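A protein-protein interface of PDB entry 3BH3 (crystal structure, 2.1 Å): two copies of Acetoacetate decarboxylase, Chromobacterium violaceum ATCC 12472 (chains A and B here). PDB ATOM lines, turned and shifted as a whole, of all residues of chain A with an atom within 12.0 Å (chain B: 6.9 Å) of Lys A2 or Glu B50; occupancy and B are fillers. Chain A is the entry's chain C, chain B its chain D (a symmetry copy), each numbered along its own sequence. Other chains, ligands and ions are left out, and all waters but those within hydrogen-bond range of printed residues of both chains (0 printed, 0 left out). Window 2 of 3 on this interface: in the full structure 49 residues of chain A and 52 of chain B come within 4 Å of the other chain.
No position is printed for both chains. Of the 11 pairs that touch across the chains among the printed residues, none has its exchanged pair printed and touching as well.
The side-chain carboxylate of Glu A5 is in hydrogen-bond range of the backbone NH of Met A1 (2.9 Å). N of Lys A2 is in hydrogen-bond range of OE2 of Glu A5, 3.0 Å away. O of Gln A3 lies within hydrogen-bond range of NH1 of Arg A7 (3.1 Å). OE1 of Gln A4 is in hydrogen-bond range of NH1 of Arg A7 (2.9 Å). The backbone carbonyl oxygen of Glu B50 is in hydrogen-bond range of the side-chain hydroxyl of Tyr B243, at 2.6 Å. O of Phe B241 lies within hydrogen-bond range of N of Leu B184 (2.7 Å).
Of the printed residues of chain B, Met A1 touches Leu B48 (3.4 Å), Pro B49 (3.9 Å) and Glu B50 (2.9 Å). Printed residues of chain B within 4 Å of Val A6: Pro B49 (3.8 Å) and Tyr B243 (3.5 Å). Of the printed residues of chain B, Arg A7 touches Tyr B243 (2.3 Å). Leu B48 touches just one residue of chain A: Met A1 (3.4 Å). Pro B49 touches just these residues of chain A: Met A1 (3.9 Å) and Val A6 (3.8 Å). Glu B50 touches three residues of chain A. Printed residues of chain A within 4 Å of Pro B51: Gln A3. Of the printed residues of chain A, Tyr B243 touches Gln A3 (3.8 Å), Val A6 (3.5 Å) and Arg A7 (2.3 Å).
Of the 10 printed residues of chain B, 6 touch a printed residue of chain A. Printed residues of chain B that touch a printed residue of chain A: Leu B48, Pro B49, Glu B50, Pro B51, Phe B241 and Tyr B243. Hydrophobic or aromatic side chains of chain B that line the printed part of chain A: Pro B49, Pro B51, Phe B241 and Tyr B243. Of the 12 printed residues of chain A, 5 touch a printed residue of chain B. Hydrophobic or aromatic side chains of chain A that line the printed part of chain B: Met A1 and Val A6. Among the printed residues, 11 pairs touch across the chains. Among the printed residues, no Asp or Glu carboxylate lies within 4 Å of a Lys or Arg side-chain nitrogen of the other chain.
Among the printed residues, pairs that only touch across the chains: Met A1 with Pro B49 (3.9 Å), Lys A2 with Glu B50 (3.96 Å), Gln A3 with Glu B50 (3.6 Å), Gln A3 with Pro B51 (3.8 Å), Gln A3 with Phe B241 (3.5 Å), Gln A3 with Tyr B243 (3.8 Å), Val A6 with Pro B49 (3.8 Å) and Val A6 with Tyr B243 (3.5 Å).
The backbone carbonyl oxygen (O) of Met A1 sits at hydrogen-bond distance from the backbone NH (N) of Glu B50 (2.9 Å). The guanidinium group (NH2) of Arg A7 sits close to the backbone carbonyl oxygen (O) of Tyr B243 (3.3 Å). The side-chain sulfur of Met A1 lies close to the backbone carbonyl oxygen of Leu B48 (3.8 Å).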
ATOM      1  N   MET A   1     -12.814  20.313 -20.367  1.00  0.00           N
ATOM      2  CA  MET A   1     -13.289  19.916 -21.734  1.00  0.00           C
ATOM      3  C   MET A   1     -13.959  18.531 -21.830  1.00  0.00           C
ATOM      4  O   MET A   1     -14.404  18.120 -22.909  1.00  0.00           O
ATOM      5  CB  MET A   1     -12.173  20.086 -22.775  1.00  0.00           C
ATOM      6  CG  MET A   1     -11.844  21.565 -23.106  1.00  0.00           C
ATOM      7  SD  MET A   1     -13.228  22.593 -23.716  1.00  0.00           S
ATOM      8  CE  MET A   1     -14.018  23.096 -22.178  1.00  0.00           C
ATOM      9  N   LYS A   2     -14.045  17.837 -20.695  1.00  0.00           N
ATOM     10  CA  LYS A   2     -14.926  16.678 -20.542  1.00  0.00           C
ATOM     11  C   LYS A   2     -16.354  17.193 -20.469  1.00  0.00           C
ATOM     12  O   LYS A   2     -16.573  18.328 -20.046  1.00  0.00           O
ATOM     13  CB  LYS A   2     -14.592  15.927 -19.256  1.00  0.00           C
ATOM     14  CG  LYS A   2     -13.377  15.032 -19.358  1.00  0.00           C
ATOM     15  CD  LYS A   2     -12.733  14.794 -17.997  1.00  0.00           C
ATOM     16  CE  LYS A   2     -11.478  13.928 -18.130  1.00  0.00           C
ATOM     17  NZ  LYS A   2     -10.526  14.107 -16.995  1.00  0.00           N
ATOM     18  N   GLN A   3     -17.322  16.364 -20.859  1.00  0.00           N
ATOM     19  CA  GLN A   3     -18.739  16.773 -20.899  1.00  0.00           C
ATOM     20  C   GLN A   3     -19.235  17.471 -19.632  1.00  0.00           C
ATOM     21  O   GLN A   3     -20.052  18.394 -19.715  1.00  0.00           O
ATOM     22  CB  GLN A   3     -19.654  15.587 -21.201  1.00  0.00           C
ATOM     23  CG  GLN A   3     -19.378  14.897 -22.519  1.00  0.00           C
ATOM     24  CD  GLN A   3     -20.230  13.660 -22.718  1.00  0.00           C
ATOM     25  OE1 GLN A   3     -19.922  12.810 -23.561  1.00  0.00           O
ATOM     26  NE2 GLN A   3     -21.311  13.546 -21.943  1.00  0.00           N
ATOM     27  N   GLN A   4     -18.748  17.023 -18.470  1.00  0.00           N
ATOM     28  CA  GLN A   4     -19.123  17.613 -17.170  1.00  0.00           C
ATOM     29  C   GLN A   4     -18.522  19.007 -16.926  1.00  0.00           C
ATOM     30  O   GLN A   4     -19.184  19.877 -16.355  1.00  0.00           O
ATOM     31  CB  GLN A   4     -18.806  16.656 -16.000  1.00  0.00           C
ATOM     32  CG  GLN A   4     -19.245  17.160 -14.598  1.00  0.00           C
ATOM     33  CD  GLN A   4     -20.779  17.277 -14.392  1.00  0.00           C
ATOM     34  OE1 GLN A   4     -21.554  17.484 -15.338  1.00  0.00           O
ATOM     35  NE2 GLN A   4     -21.206  17.153 -13.136  1.00  0.00           N
ATOM     36  N   GLU A   5     -17.280  19.210 -17.361  1.00  0.00           N
ATOM     37  CA  GLU A   5     -16.622  20.516 -17.262  1.00  0.00           C
ATOM     38  C   GLU A   5     -17.213  21.541 -18.246  1.00  0.00           C
ATOM     39  O   GLU A   5     -17.156  22.746 -18.000  1.00  0.00           O
ATOM     40  CB  GLU A   5     -15.111  20.381 -17.461  1.00  0.00           C
ATOM     41  CG  GLU A   5     -14.452  19.358 -16.528  1.00  0.00           C
ATOM     42  CD  GLU A   5     -13.015  19.005 -16.936  1.00  0.00           C
ATOM     43  OE1 GLU A   5     -12.103  19.148 -16.089  1.00  0.00           O
ATOM     44  OE2 GLU A   5     -12.796  18.585 -18.096  1.00  0.00           O
ATOM     45  N   VAL A   6     -17.777  21.056 -19.352  1.00  0.00           N
ATOM     46  CA  VAL A   6     -18.467  21.922 -20.308  1.00  0.00           C
ATOM     47  C   VAL A   6     -19.750  22.482 -19.690  1.00  0.00           C
ATOM     48  O   VAL A   6     -19.977  23.688 -19.739  1.00  0.00           O
ATOM     49  CB  VAL A   6     -18.756  21.204 -21.653  1.00  0.00           C
ATOM     50  CG1 VAL A   6     -19.717  22.016 -22.532  1.00  0.00           C
ATOM     51  CG2 VAL A   6     -17.452  20.911 -22.394  1.00  0.00           C
ATOM     52  N   ARG A   7     -20.568  21.610 -19.100  1.00  0.00           N
ATOM     53  CA  ARG A   7     -21.781  22.005 -18.365  1.00  0.00           C
ATOM     54  C   ARG A   7     -21.448  23.071 -17.311  1.00  0.00           C
ATOM     55  O   ARG A   7     -22.120  24.091 -17.203  1.00  0.00           O
ATOM     56  CB  ARG A   7     -22.389  20.769 -17.689  1.00  0.00           C
ATOM     57  CG  ARG A   7     -23.918  20.636 -17.747  1.00  0.00           C
ATOM     58  CD  ARG A   7     -24.370  19.210 -17.332  1.00  0.00           C
ATOM     59  NE  ARG A   7     -24.465  18.249 -18.454  1.00  0.00           N
ATOM     60  CZ  ARG A   7     -23.555  17.319 -18.776  1.00  0.00           C
ATOM     61  NH1 ARG A   7     -22.430  17.185 -18.078  1.00  0.00           N
ATOM     62  NH2 ARG A   7     -23.764  16.508 -19.809  1.00  0.00           N
ATOM     63  N   GLN A   8     -20.379  22.820 -16.564  1.00  0.00           N
ATOM     64  CA  GLN A   8     -19.928  23.649 -15.448  1.00  0.00           C
ATOM     65  C   GLN A   8     -19.402  25.023 -15.899  1.00  0.00           C
ATOM     66  O   GLN A   8     -19.778  26.051 -15.328  1.00  0.00           O
ATOM     67  CB  GLN A   8     -18.824  22.895 -14.700  1.00  0.00           C
ATOM     68  CG  GLN A   8     -18.968  22.823 -13.191  1.00  0.00           C
ATOM     69  CD  GLN A   8     -18.268  21.587 -12.605  1.00  0.00           C
ATOM     70  OE1 GLN A   8     -17.253  21.118 -13.131  1.00  0.00           O
ATOM     71  NE2 GLN A   8     -18.819  21.056 -11.515  1.00  0.00           N
ATOM     72  N   ARG A   9     -18.552  25.032 -16.929  1.00  0.00           N
ATOM     73  CA  ARG A   9     -17.954  26.262 -17.457  1.00  0.00           C
ATOM     74  C   ARG A   9     -18.847  27.108 -18.366  1.00  0.00           C
ATOM     75  O   ARG A   9     -18.669  28.315 -18.417  1.00  0.00           O
ATOM     76  CB  ARG A   9     -16.647  25.969 -18.191  1.00  0.00           C
ATOM     77  CG  ARG A   9     -15.434  25.861 -17.279  1.00  0.00           C
ATOM     78  CD  ARG A   9     -14.173  25.637 -18.108  1.00  0.00           C
ATOM     79  NE  ARG A   9     -13.732  26.854 -18.798  1.00  0.00           N
ATOM     80  CZ  ARG A   9     -12.866  26.879 -19.814  1.00  0.00           C
ATOM     81  NH1 ARG A   9     -12.346  25.749 -20.285  1.00  0.00           N
ATOM     82  NH2 ARG A   9     -12.523  28.039 -20.371  1.00  0.00           N
ATOM     83  N   ALA A  10     -19.780  26.497 -19.089  1.00  0.00           N
ATOM     84  CA  ALA A  10     -20.643  27.248 -20.001  1.00  0.00           C
ATOM     85  C   ALA A  10     -21.275  28.509 -19.379  1.00  0.00           C
ATOM     86  O   ALA A  10     -21.803  28.489 -18.265  1.00  0.00           O
ATOM     87  CB  ALA A  10     -21.716  26.351 -20.609  1.00  0.00           C
ATOM     88  N   LEU A  15     -17.496  29.358 -25.792  1.00  0.00           N
ATOM     89  CA  LEU A  15     -17.186  28.743 -24.510  1.00  0.00           C
ATOM     90  C   LEU A  15     -15.865  29.215 -23.872  1.00  0.00           C
ATOM     91  O   LEU A  15     -15.855  29.667 -22.728  1.00  0.00           O
ATOM     92  CB  LEU A  15     -17.198  27.210 -24.679  1.00  0.00           C
ATOM     93  CG  LEU A  15     -16.807  26.355 -23.463  1.00  0.00           C
ATOM     94  CD1 LEU A  15     -17.932  26.316 -22.413  1.00  0.00           C
ATOM     95  CD2 LEU A  15     -16.436  24.948 -23.933  1.00  0.00           C
ATOM     96  N   THR A  16     -14.769  29.116 -24.621  1.00  0.00           N
ATOM     97  CA  THR A  16     -13.426  29.400 -24.100  1.00  0.00           C
ATOM     98  C   THR A  16     -12.972  30.883 -24.116  1.00  0.00           C
ATOM     99  O   THR A  16     -11.886  31.214 -23.582  1.00  0.00           O
ATOM    100  CB  THR A  16     -12.349  28.535 -24.810  1.00  0.00           C
ATOM    101  OG1 THR A  16     -12.359  28.794 -26.230  1.00  0.00           O
ATOM    102  CG2 THR A  16     -12.593  27.016 -24.529  1.00  0.00           C
ATOM    103  N   LEU B  48     -11.559  21.987 -27.460  1.00  0.00           N
ATOM    104  CA  LEU B  48     -12.548  21.071 -28.050  1.00  0.00           C
ATOM    105  C   LEU B  48     -13.423  20.411 -26.974  1.00  0.00           C
ATOM    106  O   LEU B  48     -12.911  19.688 -26.100  1.00  0.00           O
ATOM    107  CB  LEU B  48     -11.841  20.012 -28.889  1.00  0.00           C
ATOM    108  CG  LEU B  48     -12.594  19.278 -29.986  1.00  0.00           C
ATOM    109  CD1 LEU B  48     -13.145  20.225 -31.029  1.00  0.00           C
ATOM    110  CD2 LEU B  48     -11.598  18.361 -30.614  1.00  0.00           C
ATOM    111  N   PRO B  49     -14.742  20.672 -27.023  1.00  0.00           N
ATOM    112  CA  PRO B  49     -15.658  20.150 -26.009  1.00  0.00           C
ATOM    113  C   PRO B  49     -16.109  18.732 -26.343  1.00  0.00           C
ATOM    114  O   PRO B  49     -16.697  18.505 -27.407  1.00  0.00           O
ATOM    115  CB  PRO B  49     -16.849  21.105 -26.101  1.00  0.00           C
ATOM    116  CG  PRO B  49     -16.867  21.541 -27.560  1.00  0.00           C
ATOM    117  CD  PRO B  49     -15.436  21.484 -28.042  1.00  0.00           C
ATOM    118  N   GLU B  50     -15.855  17.784 -25.447  1.00  0.00           N
ATOM    119  CA  GLU B  50     -16.396  16.431 -25.627  1.00  0.00           C
ATOM    120  C   GLU B  50     -17.935  16.501 -25.601  1.00  0.00           C
ATOM    121  O   GLU B  50     -18.491  17.369 -24.917  1.00  0.00           O
ATOM    122  CB  GLU B  50     -15.807  15.477 -24.589  1.00  0.00           C
ATOM    123  CG  GLU B  50     -14.268  15.401 -24.693  1.00  0.00           C
ATOM    124  CD  GLU B  50     -13.642  14.344 -23.781  1.00  0.00           C
ATOM    125  OE1 GLU B  50     -12.546  14.615 -23.207  1.00  0.00           O
ATOM    126  OE2 GLU B  50     -14.244  13.244 -23.651  1.00  0.00           O
ATOM    127  N   PRO B  51     -18.636  15.613 -26.341  1.00  0.00           N
ATOM    128  CA  PRO B  51     -18.222  14.397 -27.041  1.00  0.00           C
ATOM    129  C   PRO B  51     -17.535  14.605 -28.396  1.00  0.00           C
ATOM    130  O   PRO B  51     -17.247  13.616 -29.084  1.00  0.00           O
ATOM    131  CB  PRO B  51     -19.550  13.659 -27.253  1.00  0.00           C
ATOM    132  CG  PRO B  51     -20.547  14.745 -27.430  1.00  0.00           C
ATOM    133  CD  PRO B  51     -20.082  15.862 -26.513  1.00  0.00           C
ATOM    134  N   LEU B  52     -17.293  15.860 -28.792  1.00  0.00           N
ATOM    135  CA  LEU B  52     -16.495  16.129 -29.996  1.00  0.00           C
ATOM    136  C   LEU B  52     -15.094  15.558 -29.843  1.00  0.00           C
ATOM    137  O   LEU B  52     -14.463  15.665 -28.780  1.00  0.00           O
ATOM    138  CB  LEU B  52     -16.459  17.621 -30.351  1.00  0.00           C
ATOM    139  CG  LEU B  52     -17.412  18.159 -31.433  1.00  0.00           C
ATOM    140  CD1 LEU B  52     -18.618  17.276 -31.745  1.00  0.00           C
ATOM    141  CD2 LEU B  52     -17.862  19.558 -31.097  1.00  0.00           C
ATOM    142  N   GLN B  53     -14.634  14.906 -30.905  1.00  0.00           N
ATOM    143  CA  GLN B  53     -13.284  14.371 -30.928  1.00  0.00           C
ATOM    144  C   GLN B  53     -12.425  14.893 -32.077  1.00  0.00           C
ATOM    145  O   GLN B  53     -12.869  15.054 -33.225  1.00  0.00           O
ATOM    146  CB  GLN B  53     -13.290  12.840 -30.887  1.00  0.00           C
ATOM    147  CG  GLN B  53     -11.936  12.283 -30.430  1.00  0.00           C
ATOM    148  CD  GLN B  53     -12.069  11.162 -29.421  1.00  0.00           C
ATOM    149  OE1 GLN B  53     -12.242   9.992 -29.793  1.00  0.00           O
ATOM    150  NE2 GLN B  53     -11.972  11.512 -28.129  1.00  0.00           N
ATOM    151  N   PHE B  86     -17.767  13.389 -34.526  1.00  0.00           N
ATOM    152  CA  PHE B  86     -18.767  13.117 -33.514  1.00  0.00           C
ATOM    153  C   PHE B  86     -19.496  11.789 -33.856  1.00  0.00           C
ATOM    154  O   PHE B  86     -20.088  11.651 -34.937  1.00  0.00           O
ATOM    155  CB  PHE B  86     -19.734  14.285 -33.456  1.00  0.00           C
ATOM    156  CG  PHE B  86     -20.948  14.048 -32.605  1.00  0.00           C
ATOM    157  CD1 PHE B  86     -22.215  13.964 -33.194  1.00  0.00           C
ATOM    158  CD2 PHE B  86     -20.840  13.933 -31.227  1.00  0.00           C
ATOM    159  CE1 PHE B  86     -23.350  13.763 -32.416  1.00  0.00           C
ATOM    160  CE2 PHE B  86     -21.978  13.727 -30.446  1.00  0.00           C
ATOM    161  CZ  PHE B  86     -23.222  13.641 -31.035  1.00  0.00           C
ATOM    162  N   LEU B 184     -24.920  20.739 -28.555  1.00  0.00           N
ATOM    163  CA  LEU B 184     -24.236  20.620 -29.847  1.00  0.00           C
ATOM    164  C   LEU B 184     -25.238  20.589 -30.976  1.00  0.00           C
ATOM    165  O   LEU B 184     -26.238  19.849 -30.935  1.00  0.00           O
ATOM    166  CB  LEU B 184     -23.362  19.361 -29.941  1.00  0.00           C
ATOM    167  CG  LEU B 184     -22.056  19.273 -29.158  1.00  0.00           C
ATOM    168  CD1 LEU B 184     -21.465  17.858 -29.317  1.00  0.00           C
ATOM    169  CD2 LEU B 184     -21.044  20.316 -29.608  1.00  0.00           C
ATOM    170  N   PHE B 241     -26.638  16.728 -29.591  1.00  0.00           N
ATOM    171  CA  PHE B 241     -26.305  16.455 -28.196  1.00  0.00           C
ATOM    172  C   PHE B 241     -26.772  17.613 -27.301  1.00  0.00           C
ATOM    173  O   PHE B 241     -26.447  18.770 -27.561  1.00  0.00           O
ATOM    174  CB  PHE B 241     -24.810  16.181 -28.000  1.00  0.00           C
ATOM    175  CG  PHE B 241     -24.458  15.719 -26.603  1.00  0.00           C
ATOM    176  CD1 PHE B 241     -24.808  14.436 -26.161  1.00  0.00           C
ATOM    177  CD2 PHE B 241     -23.781  16.559 -25.720  1.00  0.00           C
ATOM    178  CE1 PHE B 241     -24.492  14.006 -24.854  1.00  0.00           C
ATOM    179  CE2 PHE B 241     -23.451  16.136 -24.408  1.00  0.00           C
ATOM    180  CZ  PHE B 241     -23.809  14.860 -23.976  1.00  0.00           C
ATOM    181  N   TYR B 243     -26.396  18.975 -23.627  1.00  0.00           N
ATOM    182  CA  TYR B 243     -25.678  18.908 -22.351  1.00  0.00           C
ATOM    183  C   TYR B 243     -26.573  19.068 -21.102  1.00  0.00           C
ATOM    184  O   TYR B 243     -26.139  18.782 -19.996  1.00  0.00           O
ATOM    185  CB  TYR B 243     -24.555  19.947 -22.310  1.00  0.00           C
ATOM    186  CG  TYR B 243     -23.381  19.721 -23.239  1.00  0.00           C
ATOM    187  CD1 TYR B 243     -22.179  19.205 -22.751  1.00  0.00           C
ATOM    188  CD2 TYR B 243     -23.448  20.077 -24.593  1.00  0.00           C
ATOM    189  CE1 TYR B 243     -21.074  19.013 -23.592  1.00  0.00           C
ATOM    190  CE2 TYR B 243     -22.352  19.893 -25.445  1.00  0.00           C
ATOM    191  CZ  TYR B 243     -21.167  19.363 -24.936  1.00  0.00           C
ATOM    192  OH  TYR B 243     -20.072  19.188 -25.761  1.00  0.00           O
